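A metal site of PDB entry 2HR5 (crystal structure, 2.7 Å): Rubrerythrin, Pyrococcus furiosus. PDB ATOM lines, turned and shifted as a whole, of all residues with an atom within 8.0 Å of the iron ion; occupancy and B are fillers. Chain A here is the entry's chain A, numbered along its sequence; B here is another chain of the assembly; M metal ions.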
ATOM      1  N   TYR A 109      25.766 -16.356  15.118  1.00  0.00           N
ATOM      2  CA  TYR A 109      25.479 -16.762  13.746  1.00  0.00           C
ATOM      3  C   TYR A 109      26.586 -17.634  13.188  1.00  0.00           C
ATOM      4  O   TYR A 109      26.336 -18.747  12.880  1.00  0.00           O
ATOM      5  CB  TYR A 109      25.154 -15.591  12.775  1.00  0.00           C
ATOM      6  CG  TYR A 109      23.816 -14.909  12.966  1.00  0.00           C
ATOM      7  CD1 TYR A 109      22.841 -15.412  13.837  1.00  0.00           C
ATOM      8  CD2 TYR A 109      23.509 -13.727  12.254  1.00  0.00           C
ATOM      9  CE1 TYR A 109      21.649 -14.767  13.985  1.00  0.00           C
ATOM     10  CE2 TYR A 109      22.304 -13.076  12.385  1.00  0.00           C
ATOM     11  CZ  TYR A 109      21.374 -13.606  13.235  1.00  0.00           C
ATOM     12  OH  TYR A 109      20.159 -12.926  13.366  1.00  0.00           O
ATOM     13  N   ILE A 141      22.276 -21.974   1.592  1.00  0.00           N
ATOM     14  CA  ILE A 141      22.943 -21.183   2.563  1.00  0.00           C
ATOM     15  C   ILE A 141      22.011 -20.055   2.985  1.00  0.00           C
ATOM     16  O   ILE A 141      21.542 -19.310   2.133  1.00  0.00           O
ATOM     17  CB  ILE A 141      24.234 -20.527   1.945  1.00  0.00           C
ATOM     18  CG1 ILE A 141      25.099 -21.516   1.131  1.00  0.00           C
ATOM     19  CG2 ILE A 141      24.994 -19.735   3.003  1.00  0.00           C
ATOM     20  CD1 ILE A 141      25.662 -22.726   1.935  1.00  0.00           C
ATOM     21  N   CYS A 142      21.752 -19.898   4.272  1.00  0.00           N
ATOM     22  CA  CYS A 142      20.962 -18.762   4.727  1.00  0.00           C
ATOM     23  C   CYS A 142      21.754 -17.421   4.632  1.00  0.00           C
ATOM     24  O   CYS A 142      22.858 -17.323   5.189  1.00  0.00           O
ATOM     25  CB  CYS A 142      20.536 -18.997   6.149  1.00  0.00           C
ATOM     26  SG  CYS A 142      19.766 -17.607   6.892  1.00  0.00           S
ATOM     27  N   PRO A 143      21.192 -16.398   3.927  1.00  0.00           N
ATOM     28  CA  PRO A 143      22.026 -15.267   3.641  1.00  0.00           C
ATOM     29  C   PRO A 143      22.049 -14.247   4.765  1.00  0.00           C
ATOM     30  O   PRO A 143      22.636 -13.177   4.566  1.00  0.00           O
ATOM     31  CB  PRO A 143      21.411 -14.695   2.369  1.00  0.00           C
ATOM     32  CG  PRO A 143      19.943 -14.933   2.564  1.00  0.00           C
ATOM     33  CD  PRO A 143      19.863 -16.256   3.298  1.00  0.00           C
ATOM     34  N   ILE A 144      21.401 -14.562   5.886  1.00  0.00           N
ATOM     35  CA  ILE A 144      21.410 -13.746   7.096  1.00  0.00           C
ATOM     36  C   ILE A 144      22.487 -14.231   8.078  1.00  0.00           C
ATOM     37  O   ILE A 144      23.188 -13.423   8.731  1.00  0.00           O
ATOM     38  CB  ILE A 144      20.053 -13.884   7.830  1.00  0.00           C
ATOM     39  CG1 ILE A 144      18.913 -13.589   6.867  1.00  0.00           C
ATOM     40  CG2 ILE A 144      19.977 -12.991   9.062  1.00  0.00           C
ATOM     41  CD1 ILE A 144      18.917 -12.205   6.294  1.00  0.00           C
ATOM     42  N   CYS A 145      22.623 -15.555   8.214  1.00  0.00           N
ATOM     43  CA  CYS A 145      23.428 -16.141   9.260  1.00  0.00           C
ATOM     44  C   CYS A 145      24.373 -17.162   8.665  1.00  0.00           C
ATOM     45  O   CYS A 145      25.328 -17.557   9.298  1.00  0.00           O
ATOM     46  CB  CYS A 145      22.554 -16.764  10.357  1.00  0.00           C
ATOM     47  SG  CYS A 145      21.770 -18.324   9.903  1.00  0.00           S
ATOM     48  N   GLY A 146      24.160 -17.573   7.440  1.00  0.00           N
ATOM     49  CA  GLY A 146      25.096 -18.554   6.889  1.00  0.00           C
ATOM     50  C   GLY A 146      24.873 -19.994   7.307  1.00  0.00           C
ATOM     51  O   GLY A 146      25.669 -20.819   6.959  1.00  0.00           O
ATOM     52  N   TYR A 147      23.800 -20.290   8.038  1.00  0.00           N
ATOM     53  CA  TYR A 147      23.366 -21.678   8.238  1.00  0.00           C
ATOM     54  C   TYR A 147      23.498 -22.365   6.893  1.00  0.00           C
ATOM     55  O   TYR A 147      23.143 -21.785   5.867  1.00  0.00           O
ATOM     56  CB  TYR A 147      21.873 -21.761   8.756  1.00  0.00           C
ATOM     57  CG  TYR A 147      21.208 -23.107   8.589  1.00  0.00           C
ATOM     58  CD1 TYR A 147      20.430 -23.432   7.453  1.00  0.00           C
ATOM     59  CD2 TYR A 147      21.393 -24.094   9.531  1.00  0.00           C
ATOM     60  CE1 TYR A 147      19.818 -24.738   7.328  1.00  0.00           C
ATOM     61  CE2 TYR A 147      20.828 -25.384   9.410  1.00  0.00           C
ATOM     62  CZ  TYR A 147      20.060 -25.694   8.336  1.00  0.00           C
ATOM     63  OH  TYR A 147      19.545 -26.954   8.344  1.00  0.00           O
ATOM     64  N   THR A 148      23.954 -23.614   6.930  1.00  0.00           N
ATOM     65  CA  THR A 148      24.287 -24.389   5.734  1.00  0.00           C
ATOM     66  C   THR A 148      23.664 -25.779   5.834  1.00  0.00           C
ATOM     67  O   THR A 148      23.705 -26.411   6.903  1.00  0.00           O
ATOM     68  CB  THR A 148      25.784 -24.550   5.667  1.00  0.00           C
ATOM     69  OG1 THR A 148      26.348 -23.229   5.782  1.00  0.00           O
ATOM     70  CG2 THR A 148      26.233 -25.277   4.369  1.00  0.00           C
ATOM     71  N   TYR A 156      12.323 -23.174   7.703  1.00  0.00           N
ATOM     72  CA  TYR A 156      12.892 -21.886   8.187  1.00  0.00           C
ATOM     73  C   TYR A 156      14.294 -22.164   8.709  1.00  0.00           C
ATOM     74  O   TYR A 156      14.515 -23.252   9.204  1.00  0.00           O
ATOM     75  CB  TYR A 156      12.034 -21.248   9.310  1.00  0.00           C
ATOM     76  CG  TYR A 156      10.644 -20.943   8.857  1.00  0.00           C
ATOM     77  CD1 TYR A 156      10.317 -19.681   8.305  1.00  0.00           C
ATOM     78  CD2 TYR A 156       9.651 -21.952   8.904  1.00  0.00           C
ATOM     79  CE1 TYR A 156       9.045 -19.421   7.840  1.00  0.00           C
ATOM     80  CE2 TYR A 156       8.383 -21.702   8.439  1.00  0.00           C
ATOM     81  CZ  TYR A 156       8.077 -20.464   7.927  1.00  0.00           C
ATOM     82  OH  TYR A 156       6.796 -20.259   7.514  1.00  0.00           O
ATOM     83  N   CYS A 157      15.229 -21.207   8.567  1.00  0.00           N
ATOM     84  CA  CYS A 157      16.559 -21.370   9.188  1.00  0.00           C
ATOM     85  C   CYS A 157      16.449 -21.603  10.696  1.00  0.00           C
ATOM     86  O   CYS A 157      15.772 -20.826  11.410  1.00  0.00           O
ATOM     87  CB  CYS A 157      17.429 -20.154   8.887  1.00  0.00           C
ATOM     88  SG  CYS A 157      18.981 -20.070   9.702  1.00  0.00           S
ATOM     89  N   PRO A 158      17.086 -22.677  11.190  1.00  0.00           N
ATOM     90  CA  PRO A 158      16.906 -22.945  12.593  1.00  0.00           C
ATOM     91  C   PRO A 158      17.693 -21.926  13.444  1.00  0.00           C
ATOM     92  O   PRO A 158      17.546 -21.922  14.675  1.00  0.00           O
ATOM     93  CB  PRO A 158      17.449 -24.395  12.776  1.00  0.00           C
ATOM     94  CG  PRO A 158      18.325 -24.657  11.716  1.00  0.00           C
ATOM     95  CD  PRO A 158      17.924 -23.704  10.542  1.00  0.00           C
ATOM     96  N   VAL A 159      18.519 -21.078  12.800  1.00  0.00           N
ATOM     97  CA  VAL A 159      19.266 -20.063  13.569  1.00  0.00           C
ATOM     98  C   VAL A 159      18.580 -18.657  13.656  1.00  0.00           C
ATOM     99  O   VAL A 159      18.426 -18.099  14.735  1.00  0.00           O
ATOM    100  CB  VAL A 159      20.760 -20.073  13.176  1.00  0.00           C
ATOM    101  CG1 VAL A 159      21.501 -18.905  13.786  1.00  0.00           C
ATOM    102  CG2 VAL A 159      21.343 -21.367  13.668  1.00  0.00           C
ATOM    103  N   CYS A 160      18.203 -18.097  12.530  1.00  0.00           N
ATOM    104  CA  CYS A 160      17.630 -16.800  12.622  1.00  0.00           C
ATOM    105  C   CYS A 160      16.160 -16.848  12.269  1.00  0.00           C
ATOM    106  O   CYS A 160      15.509 -15.821  12.371  1.00  0.00           O
ATOM    107  CB  CYS A 160      18.382 -15.824  11.721  1.00  0.00           C
ATOM    108  SG  CYS A 160      18.376 -16.300   9.987  1.00  0.00           S
ATOM    109  N   GLY A 161      15.620 -17.989  11.807  1.00  0.00           N
ATOM    110  CA  GLY A 161      14.186 -17.974  11.314  1.00  0.00           C
ATOM    111  C   GLY A 161      13.845 -17.450   9.867  1.00  0.00           C
ATOM    112  O   GLY A 161      12.695 -17.391   9.468  1.00  0.00           O
ATOM    113  N   ALA A 162      14.869 -17.066   9.087  1.00  0.00           N
ATOM    114  CA  ALA A 162      14.719 -16.720   7.673  1.00  0.00           C
ATOM    115  C   ALA A 162      13.962 -17.832   6.954  1.00  0.00           C
ATOM    116  O   ALA A 162      14.189 -19.017   7.242  1.00  0.00           O
ATOM    117  CB  ALA A 162      16.091 -16.511   7.034  1.00  0.00           C
ATOM    118  N   PRO A 163      12.990 -17.468   6.090  1.00  0.00           N
ATOM    119  CA  PRO A 163      12.287 -18.541   5.378  1.00  0.00           C
ATOM    120  C   PRO A 163      13.159 -19.216   4.315  1.00  0.00           C
ATOM    121  O   PRO A 163      14.046 -18.568   3.759  1.00  0.00           O
ATOM    122  CB  PRO A 163      11.039 -17.821   4.800  1.00  0.00           C
ATOM    123  CG  PRO A 163      11.342 -16.380   4.747  1.00  0.00           C
ATOM    124  CD  PRO A 163      12.381 -16.126   5.828  1.00  0.00           C
ATOM    125  N   PHE A 167      16.860 -18.693   0.941  1.00  0.00           N
ATOM    126  CA  PHE A 167      18.155 -19.397   0.921  1.00  0.00           C
ATOM    127  C   PHE A 167      18.934 -19.263  -0.392  1.00  0.00           C
ATOM    128  O   PHE A 167      18.346 -19.215  -1.413  1.00  0.00           O
ATOM    129  CB  PHE A 167      18.046 -20.873   1.269  1.00  0.00           C
ATOM    130  CG  PHE A 167      17.587 -21.161   2.710  1.00  0.00           C
ATOM    131  CD1 PHE A 167      17.416 -20.157   3.644  1.00  0.00           C
ATOM    132  CD2 PHE A 167      17.349 -22.479   3.111  1.00  0.00           C
ATOM    133  CE1 PHE A 167      17.023 -20.456   4.954  1.00  0.00           C
ATOM    134  CE2 PHE A 167      16.958 -22.809   4.427  1.00  0.00           C
ATOM    135  CZ  PHE A 167      16.795 -21.803   5.356  1.00  0.00           C
ATOM    136  N   VAL B  54      28.912 -14.340   4.195  1.00  0.00           N
ATOM    137  CA  VAL B  54      27.830 -13.876   5.061  1.00  0.00           C
ATOM    138  C   VAL B  54      28.317 -13.529   6.482  1.00  0.00           C
ATOM    139  O   VAL B  54      27.934 -12.475   7.081  1.00  0.00           O
ATOM    140  CB  VAL B  54      26.628 -14.904   5.046  1.00  0.00           C
ATOM    141  CG1 VAL B  54      25.687 -14.653   6.171  1.00  0.00           C
ATOM    142  CG2 VAL B  54      25.846 -14.811   3.752  1.00  0.00           C
HETATM  143 FE    FE M   1      19.619 -17.987   9.101  1.00  0.00          FE
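The side-chain sulfur of Cys 142 lies close to the backbone NH of Ile 144 (3.6 Å).
N of Cys 142 sits at hydrogen-bond distance from O of Tyr 147 (2.8 Å).
The backbone NH (N) of Cys 157 sits at hydrogen-bond distance from the backbone carbonyl oxygen (O) of Ala 162.
SG of Cys 157 sits close to N of Val 159 (3.3 Å).
The backbone NH (N) of Ala 162 sits close to the side-chain sulfur (SG) of Cys 160, 3.7 Å away.
SG of Cys 145 lies close to N of Tyr 147, 3.4 Å away.
Within 4 Å of the iron ion: Cys 142, Cys 145, Cys 157 and Cys 160.
SG of Cys 142 binds the iron ion, at 2.2 Å.
SG of Cys 157 is bound to the iron ion, at 2.3 Å.
SG of Cys 160 is bound to the iron ion (2.3 Å).
SG of Cys 145 binds the iron ion (2.3 Å).
The iron ion has four donor atoms within binding distance.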
